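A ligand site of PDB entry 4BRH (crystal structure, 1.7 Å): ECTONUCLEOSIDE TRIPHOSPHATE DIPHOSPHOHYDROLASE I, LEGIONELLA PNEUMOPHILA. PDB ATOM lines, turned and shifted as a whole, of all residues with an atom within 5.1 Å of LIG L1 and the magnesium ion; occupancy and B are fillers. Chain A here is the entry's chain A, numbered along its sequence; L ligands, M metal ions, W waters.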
ATOM      1  N   ASP A  16     -20.764  -9.111  -1.297  1.00  0.00           N
ATOM      2  CA  ASP A  16     -21.363  -8.901   0.039  1.00  0.00           C
ATOM      3  C   ASP A  16     -21.029 -10.154   0.838  1.00  0.00           C
ATOM      4  O   ASP A  16     -21.656 -11.192   0.629  1.00  0.00           O
ATOM      5  CB  ASP A  16     -22.898  -8.697  -0.125  1.00  0.00           C
ATOM      6  CG  ASP A  16     -23.685  -8.810   1.136  1.00  0.00           C
ATOM      7  OD1 ASP A  16     -23.161  -8.876   2.255  1.00  0.00           O
ATOM      8  OD2 ASP A  16     -24.912  -8.803   0.993  1.00  0.00           O
ATOM      9  N   ALA A  17     -20.088 -10.021   1.792  1.00  0.00           N
ATOM     10  CA  ALA A  17     -19.710 -11.201   2.624  1.00  0.00           C
ATOM     11  C   ALA A  17     -20.464 -11.045   3.940  1.00  0.00           C
ATOM     12  O   ALA A  17     -19.959 -10.534   4.953  1.00  0.00           O
ATOM     13  CB  ALA A  17     -18.175 -11.293   2.777  1.00  0.00           C
ATOM     14  N   GLY A  18     -21.748 -11.522   3.919  1.00  0.00           N
ATOM     15  CA  GLY A  18     -22.639 -11.383   5.068  1.00  0.00           C
ATOM     16  C   GLY A  18     -22.532 -12.528   6.055  1.00  0.00           C
ATOM     17  O   GLY A  18     -21.802 -13.520   5.827  1.00  0.00           O
ATOM     18  N   SER A  19     -23.229 -12.385   7.167  1.00  0.00           N
ATOM     19  CA  SER A  19     -23.117 -13.367   8.221  1.00  0.00           C
ATOM     20  C   SER A  19     -23.658 -14.715   7.799  1.00  0.00           C
ATOM     21  O   SER A  19     -23.166 -15.751   8.291  1.00  0.00           O
ATOM     22  CB  SER A  19     -23.843 -12.881   9.501  1.00  0.00           C
ATOM     23  OG  SER A  19     -25.242 -12.857   9.288  1.00  0.00           O
ATOM     24  N   THR A  20     -24.617 -14.754   6.871  1.00  0.00           N
ATOM     25  CA  THR A  20     -25.183 -16.054   6.497  1.00  0.00           C
ATOM     26  C   THR A  20     -24.681 -16.570   5.139  1.00  0.00           C
ATOM     27  O   THR A  20     -24.998 -17.736   4.760  1.00  0.00           O
ATOM     28  CB  THR A  20     -26.737 -16.036   6.504  1.00  0.00           C
ATOM     29  OG1 THR A  20     -27.226 -15.181   5.476  1.00  0.00           O
ATOM     30  CG2 THR A  20     -27.297 -15.523   7.861  1.00  0.00           C
ATOM     31  N   GLY A  21     -23.903 -15.755   4.411  1.00  0.00           N
ATOM     32  CA  GLY A  21     -23.435 -16.232   3.120  1.00  0.00           C
ATOM     33  C   GLY A  21     -22.759 -15.097   2.392  1.00  0.00           C
ATOM     34  O   GLY A  21     -22.773 -13.975   2.862  1.00  0.00           O
ATOM     35  N   ARG A  23     -22.338 -13.031  -1.447  1.00  0.00           N
ATOM     36  CA  ARG A  23     -23.080 -12.808  -2.715  1.00  0.00           C
ATOM     37  C   ARG A  23     -22.183 -11.996  -3.615  1.00  0.00           C
ATOM     38  O   ARG A  23     -21.852 -10.821  -3.305  1.00  0.00           O
ATOM     39  CB  ARG A  23     -24.383 -12.095  -2.488  1.00  0.00           C
ATOM     40  CG  ARG A  23     -25.254 -12.792  -1.437  1.00  0.00           C
ATOM     41  CD  ARG A  23     -25.173 -12.095  -0.114  1.00  0.00           C
ATOM     42  NE  ARG A  23     -25.694 -13.024   0.902  1.00  0.00           N
ATOM     43  CZ  ARG A  23     -25.835 -12.679   2.195  1.00  0.00           C
ATOM     44  NH1 ARG A  23     -25.468 -11.483   2.600  1.00  0.00           N
ATOM     45  NH2 ARG A  23     -26.309 -13.581   3.084  1.00  0.00           N
ATOM     46  N   THR A  85     -19.498  -7.910   6.356  1.00  0.00           N
ATOM     47  CA  THR A  85     -20.346  -7.162   7.313  1.00  0.00           C
ATOM     48  C   THR A  85     -20.371  -7.851   8.699  1.00  0.00           C
ATOM     49  O   THR A  85     -19.303  -8.130   9.261  1.00  0.00           O
ATOM     50  CB  THR A  85     -21.729  -6.871   6.709  1.00  0.00           C
ATOM     51  OG1 THR A  85     -22.323  -8.115   6.253  1.00  0.00           O
ATOM     52  CG2 THR A  85     -21.575  -5.980   5.439  1.00  0.00           C
ATOM     53  N   ALA A  86     -21.563  -8.005   9.259  1.00  0.00           N
ATOM     54  CA  ALA A  86     -21.637  -8.252  10.728  1.00  0.00           C
ATOM     55  C   ALA A  86     -21.049  -9.604  11.158  1.00  0.00           C
ATOM     56  O   ALA A  86     -20.581  -9.702  12.312  1.00  0.00           O
ATOM     57  CB  ALA A  86     -23.112  -8.076  11.219  1.00  0.00           C
ATOM     58  N   GLY A  87     -21.048 -10.594  10.264  1.00  0.00           N
ATOM     59  CA  GLY A  87     -20.416 -11.899  10.662  1.00  0.00           C
ATOM     60  C   GLY A  87     -18.959 -11.684  11.077  1.00  0.00           C
ATOM     61  O   GLY A  87     -18.514 -12.245  12.063  1.00  0.00           O
ATOM     62  N   ARG A  89     -17.649  -8.824  11.941  1.00  0.00           N
ATOM     63  CA  ARG A  89     -17.553  -7.879  13.072  1.00  0.00           C
ATOM     64  C   ARG A  89     -17.669  -8.588  14.433  1.00  0.00           C
ATOM     65  O   ARG A  89     -17.322  -8.006  15.466  1.00  0.00           O
ATOM     66  CB  ARG A  89     -18.545  -6.676  12.927  1.00  0.00           C
ATOM     67  CG  ARG A  89     -18.427  -5.956  11.588  1.00  0.00           C
ATOM     68  CD  ARG A  89     -19.024  -4.519  11.577  1.00  0.00           C
ATOM     69  NE  ARG A  89     -20.480  -4.528  11.631  1.00  0.00           N
ATOM     70  CZ  ARG A  89     -21.249  -4.500  10.554  1.00  0.00           C
ATOM     71  NH1 ARG A  89     -20.684  -4.497   9.343  1.00  0.00           N
ATOM     72  NH2 ARG A  89     -22.584  -4.522  10.668  1.00  0.00           N
ATOM     73  N   GLU A 126     -22.154   0.101   6.047  1.00  0.00           N
ATOM     74  CA  GLU A 126     -23.143  -0.835   5.486  1.00  0.00           C
ATOM     75  C   GLU A 126     -24.482  -0.078   5.365  1.00  0.00           C
ATOM     76  O   GLU A 126     -25.140  -0.193   4.356  1.00  0.00           O
ATOM     77  CB  GLU A 126     -23.279  -2.037   6.411  1.00  0.00           C
ATOM     78  CG  GLU A 126     -24.161  -3.162   5.891  1.00  0.00           C
ATOM     79  CD  GLU A 126     -24.143  -4.319   6.885  1.00  0.00           C
ATOM     80  OE1 GLU A 126     -23.480  -4.154   7.983  1.00  0.00           O
ATOM     81  OE2 GLU A 126     -24.811  -5.384   6.671  1.00  0.00           O
ATOM     82  N   ASP A 153     -32.258  -2.453   6.980  1.00  0.00           N
ATOM     83  CA  ASP A 153     -31.717  -3.715   6.492  1.00  0.00           C
ATOM     84  C   ASP A 153     -31.670  -4.675   7.672  1.00  0.00           C
ATOM     85  O   ASP A 153     -30.998  -4.415   8.674  1.00  0.00           O
ATOM     86  CB  ASP A 153     -30.283  -3.435   5.945  1.00  0.00           C
ATOM     87  CG  ASP A 153     -29.520  -4.676   5.504  1.00  0.00           C
ATOM     88  OD1 ASP A 153     -29.785  -5.785   5.986  1.00  0.00           O
ATOM     89  OD2 ASP A 153     -28.539  -4.509   4.730  1.00  0.00           O
ATOM     90  N   MET A 154     -32.433  -5.753   7.515  1.00  0.00           N
ATOM     91  CA  MET A 154     -32.548  -6.778   8.489  1.00  0.00           C
ATOM     92  C   MET A 154     -31.607  -7.928   8.166  1.00  0.00           C
ATOM     93  O   MET A 154     -31.933  -8.720   7.311  1.00  0.00           O
ATOM     94  CB  MET A 154     -34.001  -7.275   8.483  1.00  0.00           C
ATOM     95  CG  MET A 154     -34.991  -6.125   8.603  1.00  0.00           C
ATOM     96  SD  MET A 154     -34.866  -5.228  10.163  1.00  0.00           S
ATOM     97  CE  MET A 154     -36.411  -4.245  10.117  1.00  0.00           C
ATOM     98  N   GLY A 155     -30.466  -8.034   8.870  1.00  0.00           N
ATOM     99  CA  GLY A 155     -29.458  -9.066   8.546  1.00  0.00           C
ATOM    100  C   GLY A 155     -29.457 -10.175   9.619  1.00  0.00           C
ATOM    101  O   GLY A 155     -30.277 -10.162  10.566  1.00  0.00           O
ATOM    102  N   GLY A 156     -28.539 -11.097   9.445  1.00  0.00           N
ATOM    103  CA  GLY A 156     -28.399 -12.247  10.381  1.00  0.00           C
ATOM    104  C   GLY A 156     -27.758 -11.850  11.690  1.00  0.00           C
ATOM    105  O   GLY A 156     -28.123 -12.435  12.735  1.00  0.00           O
ATOM    106  N   ALA A 157     -26.837 -10.906  11.674  1.00  0.00           N
ATOM    107  CA  ALA A 157     -26.154 -10.545  12.927  1.00  0.00           C
ATOM    108  C   ALA A 157     -26.319  -9.083  13.299  1.00  0.00           C
ATOM    109  O   ALA A 157     -26.265  -8.754  14.450  1.00  0.00           O
ATOM    110  CB  ALA A 157     -24.672 -10.986  12.828  1.00  0.00           C
ATOM    111  N   SER A 158     -26.532  -8.214  12.296  1.00  0.00           N
ATOM    112  CA  SER A 158     -26.829  -6.793  12.590  1.00  0.00           C
ATOM    113  C   SER A 158     -28.056  -6.347  11.830  1.00  0.00           C
ATOM    114  O   SER A 158     -28.436  -6.951  10.793  1.00  0.00           O
ATOM    115  CB  SER A 158     -25.641  -5.875  12.187  1.00  0.00           C
ATOM    116  OG  SER A 158     -25.552  -5.766  10.736  1.00  0.00           O
ATOM    117  N   GLN A 160     -29.596  -2.490  10.286  1.00  0.00           N
ATOM    118  CA  GLN A 160     -29.273  -1.086  10.116  1.00  0.00           C
ATOM    119  C   GLN A 160     -30.528  -0.257   9.897  1.00  0.00           C
ATOM    120  O   GLN A 160     -31.531  -0.748   9.318  1.00  0.00           O
ATOM    121  CB  GLN A 160     -28.431  -0.837   8.849  1.00  0.00           C
ATOM    122  CG  GLN A 160     -26.978  -1.267   8.934  1.00  0.00           C
ATOM    123  CD  GLN A 160     -26.821  -2.776   8.898  1.00  0.00           C
ATOM    124  OE1 GLN A 160     -26.429  -3.354   9.911  1.00  0.00           O
ATOM    125  NE2 GLN A 160     -27.104  -3.422   7.774  1.00  0.00           N
ATOM    126  N   GLN A 198     -31.175 -11.348  13.036  1.00  0.00           N
ATOM    127  CA  GLN A 198     -32.124 -12.406  13.419  1.00  0.00           C
ATOM    128  C   GLN A 198     -31.461 -13.614  14.036  1.00  0.00           C
ATOM    129  O   GLN A 198     -32.017 -14.237  14.971  1.00  0.00           O
ATOM    130  CB  GLN A 198     -33.055 -12.755  12.257  1.00  0.00           C
ATOM    131  CG  GLN A 198     -32.432 -13.448  11.073  1.00  0.00           C
ATOM    132  CD  GLN A 198     -33.520 -13.957  10.096  1.00  0.00           C
ATOM    133  OE1 GLN A 198     -33.774 -13.268   9.123  1.00  0.00           O
ATOM    134  NE2 GLN A 198     -34.144 -15.109  10.385  1.00  0.00           N
ATOM    135  N   GLY A 265     -33.649  -7.506   3.390  1.00  0.00           N
ATOM    136  CA  GLY A 265     -33.195  -8.566   4.334  1.00  0.00           C
ATOM    137  C   GLY A 265     -34.269  -9.559   4.695  1.00  0.00           C
ATOM    138  O   GLY A 265     -35.279  -9.740   3.976  1.00  0.00           O
ATOM    139  N   GLY A 266     -34.089 -10.240   5.831  1.00  0.00           N
ATOM    140  CA  GLY A 266     -34.977 -11.347   6.175  1.00  0.00           C
ATOM    141  C   GLY A 266     -36.445 -11.049   6.240  1.00  0.00           C
ATOM    142  O   GLY A 266     -37.283 -11.918   6.057  1.00  0.00           O
ATOM    143  N   ASN A 269     -38.260 -12.120   3.165  1.00  0.00           N
ATOM    144  CA  ASN A 269     -38.535 -13.549   3.077  1.00  0.00           C
ATOM    145  C   ASN A 269     -39.701 -13.932   3.965  1.00  0.00           C
ATOM    146  O   ASN A 269     -40.548 -14.745   3.547  1.00  0.00           O
ATOM    147  CB  ASN A 269     -37.308 -14.325   3.538  1.00  0.00           C
ATOM    148  CG  ASN A 269     -36.116 -13.998   2.733  1.00  0.00           C
ATOM    149  OD1 ASN A 269     -35.524 -12.913   2.879  1.00  0.00           O
ATOM    150  ND2 ASN A 269     -35.729 -14.932   1.832  1.00  0.00           N
ATOM    151  N   LEU A 270     -39.775 -13.388   5.210  1.00  0.00           N
ATOM    152  CA  LEU A 270     -40.882 -13.698   6.110  1.00  0.00           C
ATOM    153  C   LEU A 270     -42.216 -13.293   5.464  1.00  0.00           C
ATOM    154  O   LEU A 270     -43.141 -14.100   5.372  1.00  0.00           O
ATOM    155  CB  LEU A 270     -40.717 -13.018   7.522  1.00  0.00           C
ATOM    156  CG  LEU A 270     -41.834 -13.285   8.572  1.00  0.00           C
ATOM    157  CD1 LEU A 270     -41.772 -14.739   9.020  1.00  0.00           C
ATOM    158  CD2 LEU A 270     -41.789 -12.354   9.811  1.00  0.00           C
ATOM    159  N   TYR A 313     -37.324 -21.654   7.633  1.00  0.00           N
ATOM    160  CA  TYR A 313     -37.254 -20.894   8.896  1.00  0.00           C
ATOM    161  C   TYR A 313     -38.634 -20.918   9.598  1.00  0.00           C
ATOM    162  O   TYR A 313     -38.792 -20.222  10.604  1.00  0.00           O
ATOM    163  CB  TYR A 313     -36.814 -19.434   8.646  1.00  0.00           C
ATOM    164  CG  TYR A 313     -35.323 -19.166   8.493  1.00  0.00           C
ATOM    165  CD1 TYR A 313     -34.651 -19.419   7.282  1.00  0.00           C
ATOM    166  CD2 TYR A 313     -34.611 -18.600   9.577  1.00  0.00           C
ATOM    167  CE1 TYR A 313     -33.263 -19.171   7.195  1.00  0.00           C
ATOM    168  CE2 TYR A 313     -33.245 -18.354   9.490  1.00  0.00           C
ATOM    169  CZ  TYR A 313     -32.581 -18.616   8.298  1.00  0.00           C
ATOM    170  OH  TYR A 313     -31.208 -18.302   8.272  1.00  0.00           O
ATOM    171  N   TYR A 317     -41.068 -18.558  12.813  1.00  0.00           N
ATOM    172  CA  TYR A 317     -41.957 -17.488  12.333  1.00  0.00           C
ATOM    173  C   TYR A 317     -42.726 -16.760  13.440  1.00  0.00           C
ATOM    174  O   TYR A 317     -43.035 -15.571  13.299  1.00  0.00           O
ATOM    175  CB  TYR A 317     -42.992 -18.017  11.322  1.00  0.00           C
ATOM    176  CG  TYR A 317     -42.434 -18.246   9.932  1.00  0.00           C
ATOM    177  CD1 TYR A 317     -41.049 -18.209   9.627  1.00  0.00           C
ATOM    178  CD2 TYR A 317     -43.360 -18.479   8.900  1.00  0.00           C
ATOM    179  CE1 TYR A 317     -40.608 -18.417   8.290  1.00  0.00           C
ATOM    180  CE2 TYR A 317     -42.936 -18.666   7.596  1.00  0.00           C
ATOM    181  CZ  TYR A 317     -41.558 -18.665   7.336  1.00  0.00           C
ATOM    182  OH  TYR A 317     -41.134 -18.849   6.013  1.00  0.00           O
ATOM    183  N   LEU A 320     -40.064 -14.453  14.803  1.00  0.00           N
ATOM    184  CA  LEU A 320     -39.581 -13.395  13.888  1.00  0.00           C
ATOM    185  C   LEU A 320     -40.659 -12.338  13.759  1.00  0.00           C
ATOM    186  O   LEU A 320     -40.357 -11.161  13.704  1.00  0.00           O
ATOM    187  CB  LEU A 320     -39.245 -13.986  12.526  1.00  0.00           C
ATOM    188  CG  LEU A 320     -37.971 -14.839  12.519  1.00  0.00           C
ATOM    189  CD1 LEU A 320     -37.890 -15.592  11.158  1.00  0.00           C
ATOM    190  CD2 LEU A 320     -36.708 -14.065  12.884  1.00  0.00           C
ATOM    191  N   TRP A 351     -26.871  -4.187  -0.521  1.00  0.00           N
ATOM    192  CA  TRP A 351     -26.348  -2.811  -0.501  1.00  0.00           C
ATOM    193  C   TRP A 351     -25.244  -2.618  -1.532  1.00  0.00           C
ATOM    194  O   TRP A 351     -24.681  -1.533  -1.660  1.00  0.00           O
ATOM    195  CB  TRP A 351     -25.849  -2.488   0.896  1.00  0.00           C
ATOM    196  CG  TRP A 351     -25.028  -3.656   1.471  1.00  0.00           C
ATOM    197  CD1 TRP A 351     -25.489  -4.600   2.374  1.00  0.00           C
ATOM    198  CD2 TRP A 351     -23.652  -3.997   1.205  1.00  0.00           C
ATOM    199  NE1 TRP A 351     -24.498  -5.529   2.635  1.00  0.00           N
ATOM    200  CE2 TRP A 351     -23.354  -5.171   1.966  1.00  0.00           C
ATOM    201  CE3 TRP A 351     -22.624  -3.409   0.442  1.00  0.00           C
ATOM    202  CZ2 TRP A 351     -22.108  -5.797   1.946  1.00  0.00           C
ATOM    203  CZ3 TRP A 351     -21.369  -4.064   0.406  1.00  0.00           C
ATOM    204  CH2 TRP A 351     -21.122  -5.239   1.187  1.00  0.00           C
HETATM  205  O1  LIG L   1     -26.285 -12.706   5.805  1.00  0.00           O
HETATM  206  P1  LIG L   1     -26.739 -11.353   6.167  1.00  0.00           P
HETATM  207  O2  LIG L   1     -26.512 -10.328   5.062  1.00  0.00           O
HETATM  208  O3  LIG L   1     -26.159 -10.760   7.518  1.00  0.00           O
HETATM  209  V1  LIG L   1     -25.382  -9.114   8.144  1.00  0.00           V
HETATM  210  O4  LIG L   1     -23.851  -9.765   7.889  1.00  0.00           O
HETATM  211  O5  LIG L   1     -26.353  -8.183   6.809  1.00  0.00           O
HETATM  212  O6  LIG L   1     -24.508  -7.208   8.550  1.00  0.00           O
HETATM  213  O7  LIG L   1     -25.964  -9.178   9.739  1.00  0.00           O
HETATM  214  O8  LIG L   1     -28.344 -11.470   6.344  1.00  0.00           O
HETATM  215  C1  LIG L   1     -29.136 -11.774   5.181  1.00  0.00           C
HETATM  216  C2  LIG L   1     -30.634 -11.619   5.485  1.00  0.00           C
HETATM  217  C3  LIG L   1     -31.290 -12.833   6.179  1.00  0.00           C
HETATM  218  C4  LIG L   1     -31.743 -13.944   5.331  1.00  0.00           C
HETATM  219  C5  LIG L   1     -32.256 -13.823   3.917  1.00  0.00           C
HETATM  220  N1  LIG L   1     -31.705 -15.064   5.946  1.00  0.00           N
HETATM  221  C6  LIG L   1     -30.938 -15.094   6.953  1.00  0.00           C
HETATM  222  S1  LIG L   1     -30.365 -13.595   7.481  1.00  0.00           S
HETATM  223  C7  LIG L   1     -32.465 -16.246   5.540  1.00  0.00           C
HETATM  224  C8  LIG L   1     -33.961 -16.226   5.852  1.00  0.00           C
HETATM  225  C9  LIG L   1     -34.966 -16.912   4.958  1.00  0.00           C
HETATM  226  N2  LIG L   1     -34.599 -17.514   3.797  1.00  0.00           N
HETATM  227  N3  LIG L   1     -36.268 -16.905   5.341  1.00  0.00           N
HETATM  228  C10 LIG L   1     -36.658 -16.267   6.487  1.00  0.00           C
HETATM  229  C11 LIG L   1     -38.099 -16.235   6.883  1.00  0.00           C
HETATM  230  N4  LIG L   1     -35.768 -15.644   7.289  1.00  0.00           N
HETATM  231  C12 LIG L   1     -34.442 -15.615   7.013  1.00  0.00           C
HETATM  232  O1  LG2 L   2     -27.803 -17.563  -0.015  1.00  0.00           O
HETATM  233  V1  LG2 L   2     -29.389 -17.871   0.141  1.00  0.00           V
HETATM  234  O2  LG2 L   2     -29.337 -19.735  -0.178  1.00  0.00           O
HETATM  235  O3  LG2 L   2     -29.629 -18.166   1.965  1.00  0.00           O
HETATM  236  V2  LG2 L   2     -31.336 -18.718   2.373  1.00  0.00           V
HETATM  237  O4  LG2 L   2     -31.239 -18.923   4.003  1.00  0.00           O
HETATM  238  O5  LG2 L   2     -30.326 -16.242   0.311  1.00  0.00           O
HETATM  239  V3  LG2 L   2     -32.154 -16.369   0.595  1.00  0.00           V
HETATM  240  O6  LG2 L   2     -31.649 -18.511   0.123  1.00  0.00           O
HETATM  241  O7  LG2 L   2     -32.021 -17.017   2.243  1.00  0.00           O
HETATM  242  O8  LG2 L   2     -33.954 -17.248   0.360  1.00  0.00           O
HETATM  243  O9  LG2 L   2     -32.641 -14.861   0.679  1.00  0.00           O
HETATM  244  O10 LG2 L   2     -32.208 -16.452  -1.416  1.00  0.00           O
HETATM  245  V4  LG2 L   2     -34.184 -16.734  -1.554  1.00  0.00           V
HETATM  246  O11 LG2 L   2     -35.709 -17.661  -1.612  1.00  0.00           O
HETATM  247  O12 LG2 L   2     -34.626 -15.195  -1.313  1.00  0.00           O
HETATM  248  O13 LG2 L   2     -33.736 -16.849  -3.363  1.00  0.00           O
HETATM  249  V5  LG2 L   2     -33.286 -18.553  -4.067  1.00  0.00           V
HETATM  250  O14 LG2 L   2     -32.657 -20.318  -3.928  1.00  0.00           O
HETATM  251  O15 LG2 L   2     -33.154 -18.318  -5.669  1.00  0.00           O
HETATM  252  O16 LG2 L   2     -35.008 -19.164  -3.811  1.00  0.00           O
HETATM  253  V6  LG2 L   2     -31.378 -18.108  -1.946  1.00  0.00           V
HETATM  254  O17 LG2 L   2     -31.405 -17.947  -3.612  1.00  0.00           O
HETATM  255  O18 LG2 L   2     -29.843 -17.582  -1.772  1.00  0.00           O
HETATM  256  O19 LG2 L   2     -33.327 -18.800  -1.766  1.00  0.00           O
HETATM  257  V7  LG2 L   2     -35.550 -19.483  -2.054  1.00  0.00           V
HETATM  258  O20 LG2 L   2     -37.094 -19.951  -2.168  1.00  0.00           O
HETATM  259  O21 LG2 L   2     -35.224 -19.631  -0.038  1.00  0.00           O
HETATM  260  V8  LG2 L   2     -33.645 -19.124   0.366  1.00  0.00           V
HETATM  261  O22 LG2 L   2     -33.287 -19.327   2.019  1.00  0.00           O
HETATM  262  O23 LG2 L   2     -31.072 -20.029  -1.968  1.00  0.00           O
HETATM  263  V9  LG2 L   2     -32.830 -20.949  -2.230  1.00  0.00           V
HETATM  264  O24 LG2 L   2     -34.617 -21.141  -2.128  1.00  0.00           O
HETATM  265  O25 LG2 L   2     -32.154 -22.411  -2.334  1.00  0.00           O
HETATM  266  O26 LG2 L   2     -32.878 -20.800  -0.229  1.00  0.00           O
HETATM  267  V10 LG2 L   2     -30.908 -20.586  -0.072  1.00  0.00           V
HETATM  268  O27 LG2 L   2     -30.977 -20.449   1.765  1.00  0.00           O
HETATM  269  O28 LG2 L   2     -30.594 -22.162  -0.239  1.00  0.00           O
HETATM  270 MG    MG M   1     -26.538  -8.307   4.809  1.00  0.00          MG
HETATM  271  O   HOH W   1     -32.743 -11.177   8.497  1.00  0.00           O
HETATM  272  O   HOH W   2     -29.393 -15.947   4.272  1.00  0.00           O
HETATM  273  O   HOH W   3     -24.437  -8.171   4.407  1.00  0.00           O
HETATM  274  O   HOH W   4     -36.728 -13.122   8.864  1.00  0.00           O
HETATM  275  O   HOH W   5     -28.674  -8.105   4.852  1.00  0.00           O
HETATM  276  O   HOH W   6     -27.841  -6.159   8.194  1.00  0.00           O
HETATM  277  O   HOH W   7     -26.435  -6.179   4.900  1.00  0.00           O
HETATM  278  O   HOH W   8     -29.397 -14.371   2.162  1.00  0.00           O
HETATM  279  O   HOH W   9     -26.800  -8.382   2.787  1.00  0.00           O
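O6 of LIG L1 sits close to OE2 of Glu 126 (2.6 Å). O1 of LIG L1 sits at hydrogen-bond distance from N of Thr 20, 2.8 Å away. OG1 of Thr 20 sits at hydrogen-bond distance from O1 of LIG L1, at 2.7 Å. An oxygen (O7) of LIG L1 sits close to the backbone NH (N) of Ala 157 (2.7 Å). An oxygen (O1) of LIG L1 sits at hydrogen-bond distance from the backbone NH (N) of Ser 19, at 3.4 Å. NH2 of Arg 23 lies within salt-bridge range of O1 of LIG L1. N of Gly 156 lies within hydrogen-bond range of O8 of LIG L1 (3.1 Å). The side-chain amide oxygen (OE1) of Gln 198 lies close to a sulfur (S1) of LIG L1, 3.8 Å away. ND2 of Asn 269 sits close to N2 of LIG L1 (3.4 Å).
NH2 of Arg 89 lies within salt-bridge range of OE1 of Glu 126 (2.9 Å). The side-chain hydroxyl of Thr 20 lies within hydrogen-bond range of the guanidinium group of Arg 23, at 3.0 Å. The backbone NH (N) of Ala 157 is in hydrogen-bond range of the side-chain hydroxyl (OG) of Ser 19 (3.5 Å). O of Ala 17 sits at hydrogen-bond distance from N of Thr 85, at 3.0 Å. The guanidinium group (NH2) of Arg 89 lies within hydrogen-bond range of the side-chain hydroxyl (OG) of Ser 158, at 3.2 Å. NH1 of Arg 23 lies within salt-bridge range of OD2 of Asp 16 (3.2 Å). O of Gly 156 is in hydrogen-bond range of N of Gln 198 (3.3 Å). O of Gly 265 lies close to OD1 of Asn 269, at 3.4 Å.
The side-chain hydroxyl (OG1) of Thr 85 lies close to an oxygen (O4) of LIG L1 (2.8 Å). N of Ala 86 sits close to O6 of LIG L1 (3.1 Å). O7 of LIG L1 lies close to N of Ser 158 (2.8 Å). Residues that only touch LIG L1: Gly 18, Gly 87, Arg 89, Met 154, Gly 155, Gly 266, Leu 270, Tyr 313 and Tyr 317. Within 4 Å of LIG L1: Gly 18, Ser 19, Thr 20, Arg 23, Thr 85, Ala 86, Gly 87, Arg 89, Glu 126, Met 154, Gly 155, Gly 156, Ala 157, Ser 158, Gln 198, Gly 266, Asn 269, Leu 270, Tyr 313 and Tyr 317.
Glu 126 touches the magnesium ion (OE2 to MG, 3.9 Å). Of the 28 residues printed, 1 comes within 4 Å of the magnesium ion. The nearest printed residue that does not touch the magnesium ion is Arg 23 (4.01 Å).
The magnesium ion is bound by O5 of LIG L1 (2.0 Å), O2 of LIG L1 (2.0 Å), water W9 (2.0 Å), water W7 (2.1 Å), water W3 (2.1 Å) and water W5 (2.1 Å). The magnesium ion has six donor atoms within binding distance.
Water W3 lies within hydrogen-bond range of the side-chain carboxylate (OD1) of Asp 16 (2.6 Å), the side-chain hydroxyl (OG1) of Thr 85 (2.8 Å) and the indole nitrogen (NE1) of Trp 351 (3.2 Å). Water W9 bridges the side-chain carboxylate (OD2) of Asp 16 and the guanidinium group (NH1) of Arg 23. Water W7 lies within hydrogen-bond range of OE2 of Glu 126 (2.5 Å), OD2 of Asp 153 (2.7 Å) and NE1 of Trp 351 (3.1 Å).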
